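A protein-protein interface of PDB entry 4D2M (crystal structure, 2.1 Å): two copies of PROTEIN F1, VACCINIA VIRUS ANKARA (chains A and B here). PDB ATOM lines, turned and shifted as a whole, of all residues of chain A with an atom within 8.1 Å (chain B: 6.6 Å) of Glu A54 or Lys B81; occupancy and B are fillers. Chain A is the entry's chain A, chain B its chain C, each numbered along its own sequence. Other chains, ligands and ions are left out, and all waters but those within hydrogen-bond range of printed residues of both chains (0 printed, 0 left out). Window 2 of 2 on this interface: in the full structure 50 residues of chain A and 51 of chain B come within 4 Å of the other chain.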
ATOM      1  N   LEU A  51     -33.352 -14.396  12.862  1.00  0.00           N
ATOM      2  CA  LEU A  51     -32.183 -14.713  12.047  1.00  0.00           C
ATOM      3  C   LEU A  51     -31.155 -13.587  12.106  1.00  0.00           C
ATOM      4  O   LEU A  51     -30.926 -12.894  11.114  1.00  0.00           O
ATOM      5  CB  LEU A  51     -32.601 -14.963  10.595  1.00  0.00           C
ATOM      6  CG  LEU A  51     -33.605 -16.091  10.349  1.00  0.00           C
ATOM      7  CD1 LEU A  51     -34.040 -16.098   8.894  1.00  0.00           C
ATOM      8  CD2 LEU A  51     -33.015 -17.435  10.731  1.00  0.00           C
ATOM      9  N   SER A  52     -30.534 -13.411  13.268  1.00  0.00           N
ATOM     10  CA  SER A  52     -29.607 -12.301  13.484  1.00  0.00           C
ATOM     11  C   SER A  52     -28.168 -12.664  13.125  1.00  0.00           C
ATOM     12  O   SER A  52     -27.489 -11.913  12.424  1.00  0.00           O
ATOM     13  CB  SER A  52     -29.674 -11.836  14.940  1.00  0.00           C
ATOM     14  OG  SER A  52     -30.954 -11.313  15.248  1.00  0.00           O
ATOM     15  N   THR A  53     -27.709 -13.812  13.613  1.00  0.00           N
ATOM     16  CA  THR A  53     -26.344 -14.273  13.370  1.00  0.00           C
ATOM     17  C   THR A  53     -26.328 -15.394  12.341  1.00  0.00           C
ATOM     18  O   THR A  53     -27.373 -15.946  12.000  1.00  0.00           O
ATOM     19  CB  THR A  53     -25.686 -14.792  14.658  1.00  0.00           C
ATOM     20  OG1 THR A  53     -26.390 -15.950  15.120  1.00  0.00           O
ATOM     21  CG2 THR A  53     -25.695 -13.724  15.741  1.00  0.00           C
ATOM     22  N   GLU A  54     -25.136 -15.731  11.857  1.00  0.00           N
ATOM     23  CA  GLU A  54     -24.965 -16.869  10.961  1.00  0.00           C
ATOM     24  C   GLU A  54     -25.435 -18.153  11.638  1.00  0.00           C
ATOM     25  O   GLU A  54     -25.998 -19.038  10.994  1.00  0.00           O
ATOM     26  CB  GLU A  54     -23.503 -17.010  10.539  1.00  0.00           C
ATOM     27  CG  GLU A  54     -23.016 -15.935   9.580  1.00  0.00           C
ATOM     28  CD  GLU A  54     -23.578 -16.098   8.180  1.00  0.00           C
ATOM     29  OE1 GLU A  54     -24.348 -17.054   7.948  1.00  0.00           O
ATOM     30  OE2 GLU A  54     -23.243 -15.269   7.308  1.00  0.00           O
ATOM     31  N   ARG A  55     -25.196 -18.244  12.943  1.00  0.00           N
ATOM     32  CA  ARG A  55     -25.606 -19.411  13.717  1.00  0.00           C
ATOM     33  C   ARG A  55     -27.122 -19.579  13.678  1.00  0.00           C
ATOM     34  O   ARG A  55     -27.623 -20.683  13.475  1.00  0.00           O
ATOM     35  CB  ARG A  55     -25.121 -19.295  15.163  1.00  0.00           C
ATOM     36  CG  ARG A  55     -25.506 -20.484  16.037  1.00  0.00           C
ATOM     37  CD  ARG A  55     -24.648 -20.570  17.291  1.00  0.00           C
ATOM     38  NE  ARG A  55     -24.832 -21.840  17.996  1.00  0.00           N
ATOM     39  CZ  ARG A  55     -25.660 -22.034  19.021  1.00  0.00           C
ATOM     40  NH1 ARG A  55     -26.404 -21.041  19.497  1.00  0.00           N
ATOM     41  NH2 ARG A  55     -25.743 -23.234  19.581  1.00  0.00           N
ATOM     42  N   ASP A  56     -27.846 -18.479  13.862  1.00  0.00           N
ATOM     43  CA  ASP A  56     -29.303 -18.506  13.810  1.00  0.00           C
ATOM     44  C   ASP A  56     -29.791 -19.010  12.454  1.00  0.00           C
ATOM     45  O   ASP A  56     -30.758 -19.769  12.376  1.00  0.00           O
ATOM     46  CB  ASP A  56     -29.880 -17.116  14.084  1.00  0.00           C
ATOM     47  CG  ASP A  56     -29.668 -16.664  15.518  1.00  0.00           C
ATOM     48  OD1 ASP A  56     -29.641 -17.525  16.421  1.00  0.00           O
ATOM     49  OD2 ASP A  56     -29.532 -15.441  15.740  1.00  0.00           O
ATOM     50  N   HIS A  57     -29.119 -18.581  11.389  1.00  0.00           N
ATOM     51  CA  HIS A  57     -29.467 -19.014  10.039  1.00  0.00           C
ATOM     52  C   HIS A  57     -29.240 -20.512   9.863  1.00  0.00           C
ATOM     53  O   HIS A  57     -30.112 -21.226   9.370  1.00  0.00           O
ATOM     54  CB  HIS A  57     -28.653 -18.248   8.996  1.00  0.00           C
ATOM     55  CG  HIS A  57     -29.168 -16.871   8.714  1.00  0.00           C
ATOM     56  ND1 HIS A  57     -30.151 -16.621   7.780  1.00  0.00           N
ATOM     57  CD2 HIS A  57     -28.826 -15.667   9.231  1.00  0.00           C
ATOM     58  CE1 HIS A  57     -30.396 -15.324   7.738  1.00  0.00           C
ATOM     59  NE2 HIS A  57     -29.606 -14.723   8.609  1.00  0.00           N
ATOM     60  N   VAL A  58     -28.064 -20.984  10.262  1.00  0.00           N
ATOM     61  CA  VAL A  58     -27.712 -22.382  10.072  1.00  0.00           C
ATOM     62  C   VAL A  58     -28.621 -23.237  10.944  1.00  0.00           C
ATOM     63  O   VAL A  58     -29.137 -24.258  10.493  1.00  0.00           O
ATOM     64  CB  VAL A  58     -26.221 -22.643  10.400  1.00  0.00           C
ATOM     65  CG1 VAL A  58     -25.869 -24.141  10.258  1.00  0.00           C
ATOM     66  CG2 VAL A  58     -25.327 -21.747   9.514  1.00  0.00           C
ATOM     67  N   MET A  59     -28.847 -22.799  12.178  1.00  0.00           N
ATOM     68  CA  MET A  59     -29.732 -23.523  13.084  1.00  0.00           C
ATOM     69  C   MET A  59     -31.136 -23.657  12.506  1.00  0.00           C
ATOM     70  O   MET A  59     -31.741 -24.728  12.564  1.00  0.00           O
ATOM     71  CB  MET A  59     -29.806 -22.826  14.440  1.00  0.00           C
ATOM     72  CG  MET A  59     -28.738 -23.270  15.430  1.00  0.00           C
ATOM     73  SD  MET A  59     -29.055 -22.721  17.123  1.00  0.00           S
ATOM     74  CE  MET A  59     -30.701 -23.373  17.372  1.00  0.00           C
ATOM     75  N   MET A  60     -31.652 -22.559  11.962  1.00  0.00           N
ATOM     76  CA  MET A  60     -32.954 -22.564  11.304  1.00  0.00           C
ATOM     77  C   MET A  60     -32.966 -23.559  10.149  1.00  0.00           C
ATOM     78  O   MET A  60     -33.960 -24.248   9.921  1.00  0.00           O
ATOM     79  CB  MET A  60     -33.304 -21.166  10.790  1.00  0.00           C
ATOM     80  CG  MET A  60     -34.637 -21.086  10.052  1.00  0.00           C
ATOM     81  SD  MET A  60     -36.064 -21.358  11.127  1.00  0.00           S
ATOM     82  CE  MET A  60     -36.201 -19.752  11.906  1.00  0.00           C
ATOM     83  N   ALA A  61     -31.856 -23.620   9.421  1.00  0.00           N
ATOM     84  CA  ALA A  61     -31.741 -24.508   8.270  1.00  0.00           C
ATOM     85  C   ALA A  61     -31.768 -25.975   8.695  1.00  0.00           C
ATOM     86  O   ALA A  61     -32.381 -26.811   8.029  1.00  0.00           O
ATOM     87  CB  ALA A  61     -30.464 -24.206   7.496  1.00  0.00           C
ATOM     88  N   LEU B  78     -38.269 -17.209   4.436  1.00  0.00           N
ATOM     89  CA  LEU B  78     -36.825 -17.285   4.641  1.00  0.00           C
ATOM     90  C   LEU B  78     -36.063 -16.497   3.579  1.00  0.00           C
ATOM     91  O   LEU B  78     -36.440 -16.508   2.408  1.00  0.00           O
ATOM     92  CB  LEU B  78     -36.349 -18.740   4.638  1.00  0.00           C
ATOM     93  CG  LEU B  78     -36.790 -19.634   5.803  1.00  0.00           C
ATOM     94  CD1 LEU B  78     -36.090 -20.980   5.722  1.00  0.00           C
ATOM     95  CD2 LEU B  78     -36.535 -18.983   7.157  1.00  0.00           C
ATOM     96  N   PRO B  79     -34.985 -15.804   3.987  1.00  0.00           N
ATOM     97  CA  PRO B  79     -34.141 -15.107   3.009  1.00  0.00           C
ATOM     98  C   PRO B  79     -33.255 -16.069   2.218  1.00  0.00           C
ATOM     99  O   PRO B  79     -33.098 -17.224   2.615  1.00  0.00           O
ATOM    100  CB  PRO B  79     -33.298 -14.171   3.880  1.00  0.00           C
ATOM    101  CG  PRO B  79     -33.225 -14.855   5.198  1.00  0.00           C
ATOM    102  CD  PRO B  79     -34.541 -15.553   5.371  1.00  0.00           C
ATOM    103  N   THR B  80     -32.685 -15.584   1.118  1.00  0.00           N
ATOM    104  CA  THR B  80     -31.858 -16.398   0.227  1.00  0.00           C
ATOM    105  C   THR B  80     -30.760 -17.151   0.975  1.00  0.00           C
ATOM    106  O   THR B  80     -30.492 -18.318   0.688  1.00  0.00           O
ATOM    107  CB  THR B  80     -31.210 -15.523  -0.869  1.00  0.00           C
ATOM    108  OG1 THR B  80     -32.236 -14.939  -1.680  1.00  0.00           O
ATOM    109  CG2 THR B  80     -30.271 -16.341  -1.759  1.00  0.00           C
ATOM    110  N   LYS B  81     -30.133 -16.474   1.931  1.00  0.00           N
ATOM    111  CA  LYS B  81     -29.050 -17.061   2.712  1.00  0.00           C
ATOM    112  C   LYS B  81     -29.496 -18.341   3.412  1.00  0.00           C
ATOM    113  O   LYS B  81     -28.830 -19.373   3.318  1.00  0.00           O
ATOM    114  CB  LYS B  81     -28.532 -16.051   3.739  1.00  0.00           C
ATOM    115  CG  LYS B  81     -27.711 -16.668   4.864  1.00  0.00           C
ATOM    116  CD  LYS B  81     -27.060 -15.609   5.739  1.00  0.00           C
ATOM    117  CE  LYS B  81     -25.892 -14.942   5.036  1.00  0.00           C
ATOM    118  NZ  LYS B  81     -25.139 -14.044   5.950  1.00  0.00           N
ATOM    119  N   THR B  82     -30.622 -18.270   4.113  1.00  0.00           N
ATOM    120  CA  THR B  82     -31.114 -19.416   4.866  1.00  0.00           C
ATOM    121  C   THR B  82     -31.546 -20.537   3.922  1.00  0.00           C
ATOM    122  O   THR B  82     -31.355 -21.715   4.220  1.00  0.00           O
ATOM    123  CB  THR B  82     -32.293 -19.030   5.775  1.00  0.00           C
ATOM    124  OG1 THR B  82     -32.026 -17.766   6.398  1.00  0.00           O
ATOM    125  CG2 THR B  82     -32.509 -20.086   6.849  1.00  0.00           C
ATOM    126  N   ARG B  83     -32.116 -20.167   2.780  1.00  0.00           N
ATOM    127  CA  ARG B  83     -32.541 -21.148   1.786  1.00  0.00           C
ATOM    128  C   ARG B  83     -31.343 -21.903   1.221  1.00  0.00           C
ATOM    129  O   ARG B  83     -31.427 -23.101   0.938  1.00  0.00           O
ATOM    130  CB  ARG B  83     -33.317 -20.469   0.655  1.00  0.00           C
ATOM    131  CG  ARG B  83     -34.627 -19.849   1.107  1.00  0.00           C
ATOM    132  CD  ARG B  83     -35.409 -19.255  -0.053  1.00  0.00           C
ATOM    133  NE  ARG B  83     -36.687 -18.706   0.395  1.00  0.00           N
ATOM    134  CZ  ARG B  83     -37.682 -18.350  -0.413  1.00  0.00           C
ATOM    135  NH1 ARG B  83     -37.561 -18.482  -1.727  1.00  0.00           N
ATOM    136  NH2 ARG B  83     -38.805 -17.865   0.098  1.00  0.00           N
ATOM    137  N   SER B  84     -30.229 -21.195   1.059  1.00  0.00           N
ATOM    138  CA  SER B  84     -28.994 -21.799   0.573  1.00  0.00           C
ATOM    139  C   SER B  84     -28.474 -22.840   1.559  1.00  0.00           C
ATOM    140  O   SER B  84     -28.009 -23.907   1.159  1.00  0.00           O
ATOM    141  CB  SER B  84     -27.925 -20.731   0.340  1.00  0.00           C
ATOM    142  OG  SER B  84     -28.378 -19.741  -0.568  1.00  0.00           O
ATOM    143  N   TYR B  85     -28.555 -22.523   2.849  1.00  0.00           N
ATOM    144  CA  TYR B  85     -28.044 -23.412   3.887  1.00  0.00           C
ATOM    145  C   TYR B  85     -28.867 -24.692   3.954  1.00  0.00           C
ATOM    146  O   TYR B  85     -28.319 -25.784   4.103  1.00  0.00           O
ATOM    147  CB  TYR B  85     -28.045 -22.715   5.250  1.00  0.00           C
ATOM    148  CG  TYR B  85     -27.141 -21.501   5.334  1.00  0.00           C
ATOM    149  CD1 TYR B  85     -26.282 -21.168   4.291  1.00  0.00           C
ATOM    150  CD2 TYR B  85     -27.145 -20.690   6.461  1.00  0.00           C
ATOM    151  CE1 TYR B  85     -25.459 -20.062   4.370  1.00  0.00           C
ATOM    152  CE2 TYR B  85     -26.324 -19.584   6.548  1.00  0.00           C
ATOM    153  CZ  TYR B  85     -25.483 -19.275   5.500  1.00  0.00           C
ATOM    154  OH  TYR B  85     -24.664 -18.174   5.578  1.00  0.00           O
ATOM    155  N   ILE B  86     -30.184 -24.548   3.846  1.00  0.00           N
ATOM    156  CA  ILE B  86     -31.080 -25.699   3.815  1.00  0.00           C
ATOM    157  C   ILE B  86     -30.691 -26.618   2.663  1.00  0.00           C
ATOM    158  O   ILE B  86     -30.596 -27.835   2.829  1.00  0.00           O
ATOM    159  CB  ILE B  86     -32.559 -25.263   3.669  1.00  0.00           C
ATOM    160  CG1 ILE B  86     -33.008 -24.511   4.925  1.00  0.00           C
ATOM    161  CG2 ILE B  86     -33.469 -26.473   3.437  1.00  0.00           C
ATOM    162  CD1 ILE B  86     -34.337 -23.794   4.785  1.00  0.00           C
ATOM    163  N   VAL B 175     -21.024 -24.026  11.943  1.00  0.00           N
ATOM    164  CA  VAL B 175     -21.411 -22.775  11.301  1.00  0.00           C
ATOM    165  C   VAL B 175     -20.332 -22.335  10.319  1.00  0.00           C
ATOM    166  O   VAL B 175     -20.636 -21.797   9.256  1.00  0.00           O
ATOM    167  CB  VAL B 175     -21.665 -21.654  12.341  1.00  0.00           C
ATOM    168  CG1 VAL B 175     -21.926 -20.311  11.658  1.00  0.00           C
ATOM    169  CG2 VAL B 175     -22.836 -22.017  13.229  1.00  0.00           C
ATOM    170  N   THR B 179     -21.023 -21.976   6.146  1.00  0.00           N
ATOM    171  CA  THR B 179     -20.814 -20.646   5.583  1.00  0.00           C
ATOM    172  C   THR B 179     -19.703 -20.657   4.533  1.00  0.00           C
ATOM    173  O   THR B 179     -19.725 -19.862   3.593  1.00  0.00           O
ATOM    174  CB  THR B 179     -20.475 -19.614   6.676  1.00  0.00           C
ATOM    175  OG1 THR B 179     -19.382 -20.089   7.472  1.00  0.00           O
ATOM    176  CG2 THR B 179     -21.686 -19.363   7.565  1.00  0.00           C
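The side-chain carboxylate of Glu A54 lies within salt-bridge range of the side-chain amino group of Lys B81 (2.6 Å). OE1 of Glu A54 lies within hydrogen-bond range of OH of Tyr B85 (2.6 Å). ND1 of His A57 lies within hydrogen-bond range of OG1 of Thr B82 (2.6 Å).
O of Leu A51 lies within hydrogen-bond range of NE2 of His A57 (3.4 Å). The backbone NH (N) of Arg A55 sits close to the side-chain hydroxyl (OG1) of Thr A53, at 3.4 Å. The side-chain hydroxyl of Thr B179 lies within hydrogen-bond range of the backbone carbonyl oxygen of Val B175.
Pro B79 touches Leu A51 (CD to CD1, 3.6 Å). CD1 of Leu A51 touches OG1 of Thr B82, 3.6 Å away. Glu A54 touches Val B175. OE1 of Glu A54 touches CG2 of Thr B179 (3.5 Å). Val B175 touches Arg A55. Pro B79 touches His A57 (CG to CE1, 3.8 Å). His A57 touches Lys B81 (ND1 to CG, 3.8 Å). CG2 of Val A58 touches CD2 of Tyr B85, 3.7 Å away. Met A60 touches Thr B82. CB of Ala A61 touches CB of Tyr B85, 3.6 Å away.
Printed residues of chain B within 4 Å of Glu A54: Lys B81, Tyr B85, Val B175 and Thr B179. Of chain A, only Glu A54 (2.6 Å) and His A57 (3.8 Å) come within 4 Å of Lys B81. Of the printed residues of chain A, Val B175 touches Glu A54 (3.8 Å) and Arg A55 (3.8 Å). Printed residues of chain B within 4 Å of Arg A55: Val B175 (3.8 Å). Of the printed residues of chain B, Leu A51 touches Pro B79 (3.6 Å) and Thr B82 (3.6 Å). The nearest residue of chain A that does not touch Lys B81 is Thr A53 (6.3 Å). The nearest printed residue of chain B that does not touch His A57 is Ile B86 (6.2 Å).
Of the 11 printed residues of chain B, 7 touch a printed residue of chain A. Of the 11 printed residues of chain A, 7 touch a printed residue of chain B. Hydrophobic or aromatic side chains of chain A that line the printed part of chain B: Leu A51, His A57, Val A58, Met A60 and Ala A61. Among the printed residues, 15 pairs touch across the chains. Among the printed residues, Asp or Glu carboxylates within 4 Å of a Lys or Arg side-chain nitrogen of the other chain: Glu A54 with Lys B81.
No position is printed for both chains.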
